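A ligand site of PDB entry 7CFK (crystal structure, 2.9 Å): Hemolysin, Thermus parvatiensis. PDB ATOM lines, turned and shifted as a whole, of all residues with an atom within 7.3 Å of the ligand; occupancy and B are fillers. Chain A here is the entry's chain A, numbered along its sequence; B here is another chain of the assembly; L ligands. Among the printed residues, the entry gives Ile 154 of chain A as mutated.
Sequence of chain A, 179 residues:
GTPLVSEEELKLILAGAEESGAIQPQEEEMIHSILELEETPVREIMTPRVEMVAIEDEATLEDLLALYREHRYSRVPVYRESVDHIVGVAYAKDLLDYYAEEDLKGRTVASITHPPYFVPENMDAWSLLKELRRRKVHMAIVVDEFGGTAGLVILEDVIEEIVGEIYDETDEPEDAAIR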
ATOM      1  N   THR A  47      35.561  30.390 -16.205  1.00  0.00           N
ATOM      2  CA  THR A  47      35.561  30.170 -17.632  1.00  0.00           C
ATOM      3  C   THR A  47      36.056  31.436 -18.316  1.00  0.00           C
ATOM      4  O   THR A  47      35.469  32.511 -18.095  1.00  0.00           O
ATOM      5  CB  THR A  47      34.163  29.833 -18.135  1.00  0.00           C
ATOM      6  OG1 THR A  47      33.752  28.553 -17.655  1.00  0.00           O
ATOM      7  CG2 THR A  47      34.152  29.838 -19.649  1.00  0.00           C
ATOM      8  N   PRO A  48      37.105  31.361 -19.137  1.00  0.00           N
ATOM      9  CA  PRO A  48      37.690  32.556 -19.761  1.00  0.00           C
ATOM     10  C   PRO A  48      36.996  32.912 -21.067  1.00  0.00           C
ATOM     11  O   PRO A  48      36.282  32.088 -21.649  1.00  0.00           O
ATOM     12  CB  PRO A  48      39.133  32.099 -20.005  1.00  0.00           C
ATOM     13  CG  PRO A  48      38.984  30.604 -20.294  1.00  0.00           C
ATOM     14  CD  PRO A  48      37.750  30.118 -19.596  1.00  0.00           C
ATOM     15  N   ARG A  49      37.198  34.171 -21.522  1.00  0.00           N
ATOM     16  CA  ARG A  49      36.588  34.615 -22.786  1.00  0.00           C
ATOM     17  C   ARG A  49      36.567  33.599 -23.902  1.00  0.00           C
ATOM     18  O   ARG A  49      35.556  33.472 -24.603  1.00  0.00           O
ATOM     19  CB  ARG A  49      37.292  35.824 -23.400  1.00  0.00           C
ATOM     20  CG  ARG A  49      36.964  37.205 -23.048  1.00  0.00           C
ATOM     21  CD  ARG A  49      38.040  37.908 -23.844  1.00  0.00           C
ATOM     22  NE  ARG A  49      39.272  37.668 -23.100  1.00  0.00           N
ATOM     23  CZ  ARG A  49      40.508  37.771 -23.564  1.00  0.00           C
ATOM     24  NH1 ARG A  49      40.740  37.995 -24.854  1.00  0.00           N
ATOM     25  NH2 ARG A  49      41.521  37.540 -22.718  1.00  0.00           N
ATOM     26  N   GLU A  51      36.450  30.532 -24.143  1.00  0.00           N
ATOM     27  CA  GLU A  51      35.469  29.473 -23.991  1.00  0.00           C
ATOM     28  C   GLU A  51      34.055  29.997 -23.749  1.00  0.00           C
ATOM     29  O   GLU A  51      33.158  29.206 -23.449  1.00  0.00           O
ATOM     30  CB  GLU A  51      35.871  28.563 -22.836  1.00  0.00           C
ATOM     31  CG  GLU A  51      37.143  27.796 -23.055  1.00  0.00           C
ATOM     32  CD  GLU A  51      37.188  26.496 -22.252  1.00  0.00           C
ATOM     33  OE1 GLU A  51      36.313  25.626 -22.486  1.00  0.00           O
ATOM     34  OE2 GLU A  51      38.084  26.329 -21.390  1.00  0.00           O
ATOM     35  N   MET A  52      33.830  31.305 -23.889  1.00  0.00           N
ATOM     36  CA  MET A  52      32.611  31.956 -23.427  1.00  0.00           C
ATOM     37  C   MET A  52      31.594  32.094 -24.567  1.00  0.00           C
ATOM     38  O   MET A  52      31.953  32.188 -25.740  1.00  0.00           O
ATOM     39  CB  MET A  52      32.949  33.334 -22.877  1.00  0.00           C
ATOM     40  CG  MET A  52      31.907  33.968 -21.997  1.00  0.00           C
ATOM     41  SD  MET A  52      32.305  35.689 -21.583  1.00  0.00           S
ATOM     42  CE  MET A  52      33.755  35.553 -20.577  1.00  0.00           C
ATOM     43  N   VAL A  53      30.319  32.122 -24.214  1.00  0.00           N
ATOM     44  CA  VAL A  53      29.216  32.327 -25.156  1.00  0.00           C
ATOM     45  C   VAL A  53      28.441  33.564 -24.736  1.00  0.00           C
ATOM     46  O   VAL A  53      27.788  33.565 -23.684  1.00  0.00           O
ATOM     47  CB  VAL A  53      28.281  31.116 -25.198  1.00  0.00           C
ATOM     48  CG1 VAL A  53      27.132  31.410 -26.122  1.00  0.00           C
ATOM     49  CG2 VAL A  53      29.048  29.898 -25.659  1.00  0.00           C
ATOM     50  N   ALA A  54      28.483  34.600 -25.560  1.00  0.00           N
ATOM     51  CA  ALA A  54      27.858  35.882 -25.229  1.00  0.00           C
ATOM     52  C   ALA A  54      26.992  36.365 -26.391  1.00  0.00           C
ATOM     53  O   ALA A  54      26.984  35.799 -27.492  1.00  0.00           O
ATOM     54  CB  ALA A  54      28.900  36.941 -24.853  1.00  0.00           C
ATOM     55  N   TYR A  68      20.600  29.533 -27.478  1.00  0.00           N
ATOM     56  CA  TYR A  68      20.418  28.523 -26.452  1.00  0.00           C
ATOM     57  C   TYR A  68      20.305  27.139 -27.066  1.00  0.00           C
ATOM     58  O   TYR A  68      20.869  26.172 -26.562  1.00  0.00           O
ATOM     59  CB  TYR A  68      19.192  28.816 -25.588  1.00  0.00           C
ATOM     60  CG  TYR A  68      18.901  27.689 -24.645  1.00  0.00           C
ATOM     61  CD1 TYR A  68      19.438  27.663 -23.370  1.00  0.00           C
ATOM     62  CD2 TYR A  68      18.083  26.627 -25.042  1.00  0.00           C
ATOM     63  CE1 TYR A  68      19.196  26.615 -22.526  1.00  0.00           C
ATOM     64  CE2 TYR A  68      17.836  25.581 -24.205  1.00  0.00           C
ATOM     65  CZ  TYR A  68      18.392  25.577 -22.954  1.00  0.00           C
ATOM     66  OH  TYR A  68      18.137  24.526 -22.140  1.00  0.00           O
ATOM     67  N   HIS A  71      23.783  25.925 -28.312  1.00  0.00           N
ATOM     68  CA  HIS A  71      24.892  25.813 -27.369  1.00  0.00           C
ATOM     69  C   HIS A  71      24.545  25.392 -25.939  1.00  0.00           C
ATOM     70  O   HIS A  71      25.468  25.101 -25.174  1.00  0.00           O
ATOM     71  CB  HIS A  71      25.671  27.139 -27.314  1.00  0.00           C
ATOM     72  CG  HIS A  71      26.301  27.519 -28.623  1.00  0.00           C
ATOM     73  ND1 HIS A  71      25.600  28.117 -29.640  1.00  0.00           N
ATOM     74  CD2 HIS A  71      27.572  27.392 -29.063  1.00  0.00           C
ATOM     75  CE1 HIS A  71      26.410  28.337 -30.668  1.00  0.00           C
ATOM     76  NE2 HIS A  71      27.623  27.912 -30.334  1.00  0.00           N
ATOM     77  N   ARG A  72      23.275  25.381 -25.549  1.00  0.00           N
ATOM     78  CA  ARG A  72      22.780  24.824 -24.286  1.00  0.00           C
ATOM     79  C   ARG A  72      23.201  25.608 -23.043  1.00  0.00           C
ATOM     80  O   ARG A  72      23.046  25.117 -21.933  1.00  0.00           O
ATOM     81  CB  ARG A  72      23.216  23.366 -24.084  1.00  0.00           C
ATOM     82  CG  ARG A  72      22.938  22.422 -25.235  1.00  0.00           C
ATOM     83  CD  ARG A  72      21.608  22.697 -25.881  1.00  0.00           C
ATOM     84  NE  ARG A  72      20.522  22.179 -25.063  1.00  0.00           N
ATOM     85  CZ  ARG A  72      19.307  21.891 -25.531  1.00  0.00           C
ATOM     86  NH1 ARG A  72      19.051  22.068 -26.834  1.00  0.00           N
ATOM     87  NH2 ARG A  72      18.370  21.431 -24.700  1.00  0.00           N
ATOM     88  N   TYR A  73      23.703  26.830 -23.181  1.00  0.00           N
ATOM     89  CA  TYR A  73      24.097  27.611 -22.011  1.00  0.00           C
ATOM     90  C   TYR A  73      22.945  28.471 -21.518  1.00  0.00           C
ATOM     91  O   TYR A  73      22.452  29.330 -22.264  1.00  0.00           O
ATOM     92  CB  TYR A  73      25.327  28.465 -22.307  1.00  0.00           C
ATOM     93  CG  TYR A  73      26.563  27.621 -22.396  1.00  0.00           C
ATOM     94  CD1 TYR A  73      26.900  26.756 -21.361  1.00  0.00           C
ATOM     95  CD2 TYR A  73      27.386  27.657 -23.517  1.00  0.00           C
ATOM     96  CE1 TYR A  73      28.024  25.966 -21.442  1.00  0.00           C
ATOM     97  CE2 TYR A  73      28.506  26.879 -23.604  1.00  0.00           C
ATOM     98  CZ  TYR A  73      28.833  26.037 -22.566  1.00  0.00           C
ATOM     99  OH  TYR A  73      29.951  25.250 -22.654  1.00  0.00           O
ATOM    100  N   SER A  74      22.571  28.261 -20.250  1.00  0.00           N
ATOM    101  CA  SER A  74      21.409  28.902 -19.621  1.00  0.00           C
ATOM    102  C   SER A  74      21.660  30.347 -19.232  1.00  0.00           C
ATOM    103  O   SER A  74      20.707  31.106 -19.064  1.00  0.00           O
ATOM    104  CB  SER A  74      21.032  28.118 -18.393  1.00  0.00           C
ATOM    105  OG  SER A  74      20.668  26.785 -18.751  1.00  0.00           O
ATOM    106  N   ARG A  75      22.910  30.723 -19.013  1.00  0.00           N
ATOM    107  CA  ARG A  75      23.288  32.063 -18.596  1.00  0.00           C
ATOM    108  C   ARG A  75      24.270  32.598 -19.620  1.00  0.00           C
ATOM    109  O   ARG A  75      25.202  31.911 -19.993  1.00  0.00           O
ATOM    110  CB  ARG A  75      23.926  32.018 -17.209  1.00  0.00           C
ATOM    111  CG  ARG A  75      23.376  30.884 -16.386  1.00  0.00           C
ATOM    112  CD  ARG A  75      23.591  31.102 -14.916  1.00  0.00           C
ATOM    113  NE  ARG A  75      23.623  29.830 -14.203  1.00  0.00           N
ATOM    114  CZ  ARG A  75      23.878  29.717 -12.904  1.00  0.00           C
ATOM    115  NH1 ARG A  75      24.142  30.814 -12.196  1.00  0.00           N
ATOM    116  NH2 ARG A  75      23.904  28.523 -12.337  1.00  0.00           N
ATOM    117  N   VAL A  76      24.020  33.806 -20.107  1.00  0.00           N
ATOM    118  CA  VAL A  76      24.752  34.349 -21.226  1.00  0.00           C
ATOM    119  C   VAL A  76      25.192  35.792 -20.881  1.00  0.00           C
ATOM    120  O   VAL A  76      24.357  36.636 -20.634  1.00  0.00           O
ATOM    121  CB  VAL A  76      23.911  34.371 -22.522  1.00  0.00           C
ATOM    122  CG1 VAL A  76      24.741  34.861 -23.636  1.00  0.00           C
ATOM    123  CG2 VAL A  76      23.437  32.974 -22.848  1.00  0.00           C
ATOM    124  N   PRO A  77      26.485  36.066 -20.848  1.00  0.00           N
ATOM    125  CA  PRO A  77      26.885  37.465 -20.678  1.00  0.00           C
ATOM    126  C   PRO A  77      26.391  38.247 -21.881  1.00  0.00           C
ATOM    127  O   PRO A  77      26.401  37.756 -23.012  1.00  0.00           O
ATOM    128  CB  PRO A  77      28.418  37.393 -20.625  1.00  0.00           C
ATOM    129  CG  PRO A  77      28.757  35.944 -20.471  1.00  0.00           C
ATOM    130  CD  PRO A  77      27.632  35.188 -21.107  1.00  0.00           C
ATOM    131  N   MET A 139      26.118  34.882 -11.079  1.00  0.00           N
ATOM    132  CA  MET A 139      27.213  34.830 -12.029  1.00  0.00           C
ATOM    133  C   MET A 139      27.906  36.179 -12.055  1.00  0.00           C
ATOM    134  O   MET A 139      27.232  37.215 -12.104  1.00  0.00           O
ATOM    135  CB  MET A 139      26.726  34.473 -13.433  1.00  0.00           C
ATOM    136  CG  MET A 139      27.671  34.965 -14.523  1.00  0.00           C
ATOM    137  SD  MET A 139      27.208  34.539 -16.223  1.00  0.00           S
ATOM    138  CE  MET A 139      27.429  32.758 -16.280  1.00  0.00           C
ATOM    139  N   LEU A 152      34.044  34.377 -17.075  1.00  0.00           N
ATOM    140  CA  LEU A 152      32.872  34.395 -16.193  1.00  0.00           C
ATOM    141  C   LEU A 152      32.985  33.314 -15.121  1.00  0.00           C
ATOM    142  O   LEU A 152      33.673  32.305 -15.311  1.00  0.00           O
ATOM    143  CB  LEU A 152      31.563  34.221 -16.965  1.00  0.00           C
ATOM    144  CG  LEU A 152      31.325  32.935 -17.751  1.00  0.00           C
ATOM    145  CD1 LEU A 152      30.814  31.786 -16.885  1.00  0.00           C
ATOM    146  CD2 LEU A 152      30.333  33.256 -18.847  1.00  0.00           C
ATOM    147  N   ILE A 154      30.446  31.348 -11.849  1.00  0.00           N
ATOM    148  CA  ILE A 154      29.138  31.202 -11.225  1.00  0.00           C
ATOM    149  C   ILE A 154      29.297  30.574  -9.835  1.00  0.00           C
ATOM    150  O   ILE A 154      30.330  29.991  -9.495  1.00  0.00           O
ATOM    151  CB  ILE A 154      28.150  30.378 -12.063  1.00  0.00           C
ATOM    152  CG1 ILE A 154      28.682  28.956 -12.307  1.00  0.00           C
ATOM    153  CG2 ILE A 154      27.896  31.053 -13.366  1.00  0.00           C
ATOM    154  CD1 ILE A 154      27.763  28.062 -13.065  1.00  0.00           C
ATOM    155  N   GLU A 156      27.945  27.891  -8.587  1.00  0.00           N
ATOM    156  CA  GLU A 156      28.099  26.437  -8.590  1.00  0.00           C
ATOM    157  C   GLU A 156      29.536  26.019  -8.814  1.00  0.00           C
ATOM    158  O   GLU A 156      29.896  24.892  -8.450  1.00  0.00           O
ATOM    159  CB  GLU A 156      27.194  25.820  -9.648  1.00  0.00           C
ATOM    160  CG  GLU A 156      25.719  26.159  -9.461  1.00  0.00           C
ATOM    161  CD  GLU A 156      25.370  27.644  -9.689  1.00  0.00           C
ATOM    162  OE1 GLU A 156      26.274  28.480  -9.896  1.00  0.00           O
ATOM    163  OE2 GLU A 156      24.172  28.005  -9.616  1.00  0.00           O
ATOM    164  N   ASP A 157      30.365  26.919  -9.360  1.00  0.00           N
ATOM    165  CA  ASP A 157      31.803  26.724  -9.434  1.00  0.00           C
ATOM    166  C   ASP A 157      32.405  26.622  -8.037  1.00  0.00           C
ATOM    167  O   ASP A 157      33.122  25.662  -7.707  1.00  0.00           O
ATOM    168  CB  ASP A 157      32.442  27.920 -10.133  1.00  0.00           C
ATOM    169  CG  ASP A 157      31.944  28.097 -11.553  1.00  0.00           C
ATOM    170  OD1 ASP A 157      31.524  27.097 -12.142  1.00  0.00           O
ATOM    171  OD2 ASP A 157      31.943  29.246 -12.076  1.00  0.00           O
ATOM    172  N   ILE A 166      29.450  18.529  -9.922  1.00  0.00           N
ATOM    173  CA  ILE A 166      27.998  18.376  -9.797  1.00  0.00           C
ATOM    174  C   ILE A 166      27.419  18.353 -11.219  1.00  0.00           C
ATOM    175  O   ILE A 166      27.050  19.373 -11.794  1.00  0.00           O
ATOM    176  CB  ILE A 166      27.380  19.454  -8.895  1.00  0.00           C
ATOM    177  CG1 ILE A 166      27.745  20.893  -9.332  1.00  0.00           C
ATOM    178  CG2 ILE A 166      27.744  19.204  -7.424  1.00  0.00           C
ATOM    179  CD1 ILE A 166      27.003  22.004  -8.584  1.00  0.00           C
ATOM    180  N   ASP A 168      25.169  17.873 -14.387  1.00  0.00           N
ATOM    181  CA  ASP A 168      23.762  18.149 -14.700  1.00  0.00           C
ATOM    182  C   ASP A 168      23.020  16.917 -15.226  1.00  0.00           C
ATOM    183  O   ASP A 168      21.824  16.968 -15.518  1.00  0.00           O
ATOM    184  CB  ASP A 168      23.677  19.298 -15.716  1.00  0.00           C
ATOM    185  CG  ASP A 168      23.817  20.680 -15.058  1.00  0.00           C
ATOM    186  OD1 ASP A 168      23.819  20.754 -13.812  1.00  0.00           O
ATOM    187  OD2 ASP A 168      23.950  21.681 -15.795  1.00  0.00           O
ATOM    188  N   LYS B  93      12.821  23.984 -18.458  1.00  0.00           N
ATOM    189  CA  LYS B  93      13.731  24.456 -19.511  1.00  0.00           C
ATOM    190  C   LYS B  93      13.646  23.589 -20.752  1.00  0.00           C
ATOM    191  O   LYS B  93      13.958  24.065 -21.853  1.00  0.00           O
ATOM    192  CB  LYS B  93      15.189  24.498 -19.058  1.00  0.00           C
ATOM    193  CG  LYS B  93      15.502  25.519 -17.978  1.00  0.00           C
ATOM    194  CD  LYS B  93      16.922  26.082 -18.091  1.00  0.00           C
ATOM    195  CE  LYS B  93      17.524  26.271 -16.699  1.00  0.00           C
ATOM    196  NZ  LYS B  93      18.751  27.100 -16.669  1.00  0.00           N
HETATM  197  N1  LIG L   1      28.006  31.639 -21.460  1.00  0.00           N
HETATM  198  C1  LIG L   1      25.825  26.497 -16.533  1.00  0.00           C
HETATM  199  C2  LIG L   1      24.848  25.857 -17.549  1.00  0.00           C
HETATM  200  C3  LIG L   1      25.286  26.224 -15.114  1.00  0.00           C
HETATM  201  C4  LIG L   1      29.140  28.687 -19.428  1.00  0.00           C
HETATM  202  C5  LIG L   1      28.335  29.730 -19.830  1.00  0.00           C
HETATM  203  C6  LIG L   1      28.781  30.512 -20.952  1.00  0.00           C
HETATM  204  C7  LIG L   1      27.354  28.721 -18.106  1.00  0.00           C
HETATM  205  C8  LIG L   1      30.705  29.200 -21.118  1.00  0.00           C
HETATM  206  C9  LIG L   1      25.416  24.764 -14.639  1.00  0.00           C
HETATM  207  N2  LIG L   1      28.500  28.100 -18.353  1.00  0.00           N
HETATM  208  N3  LIG L   1      30.321  28.452 -20.093  1.00  0.00           N
HETATM  209  N4  LIG L   1      27.252  29.717 -18.997  1.00  0.00           N
HETATM  210  N5  LIG L   1      29.944  30.206 -21.543  1.00  0.00           N
HETATM  211  O1  LIG L   1      25.266  24.946 -18.324  1.00  0.00           O
HETATM  212  O2  LIG L   1      23.622  26.204 -17.595  1.00  0.00           O
HETATM  213  S1  LIG L   1      26.134  28.301 -16.787  1.00  0.00           S
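A nitrogen (N5) of the ligand sits at hydrogen-bond distance from the backbone NH (N) of Val 53 (3.3 Å). The backbone carbonyl oxygen (O) of Val 53 is in hydrogen-bond range of a nitrogen (N1) of the ligand, 3.0 Å away. The backbone carbonyl oxygen of Arg 75 sits at hydrogen-bond distance from a nitrogen (N1) of the ligand. O2 of the ligand is in hydrogen-bond range of OG of Ser 74, at 3.2 Å.
The guanidinium group (NH2) of Arg 75 lies within salt-bridge range of the side-chain carboxylate (OE2) of Glu 156 (2.8 Å). OG of Ser 74 lies within hydrogen-bond range of NZ of Lys 93 of chain B (2.8 Å). OD2 of Asp 157 lies within hydrogen-bond range of N of Ile 154 (2.6 Å). N of Leu 152 lies within hydrogen-bond range of O of Thr 47 (2.6 Å).
Merely in contact with the ligand: Thr 47, Glu 51, Met 52, Tyr 73, Pro 77, Leu 152, Ile 154 and Asp 168. Hydrophobic or aromatic side chains within 4 Å of the ligand: Val 53, Tyr 73, Pro 77, Leu 152 and Ile 154.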
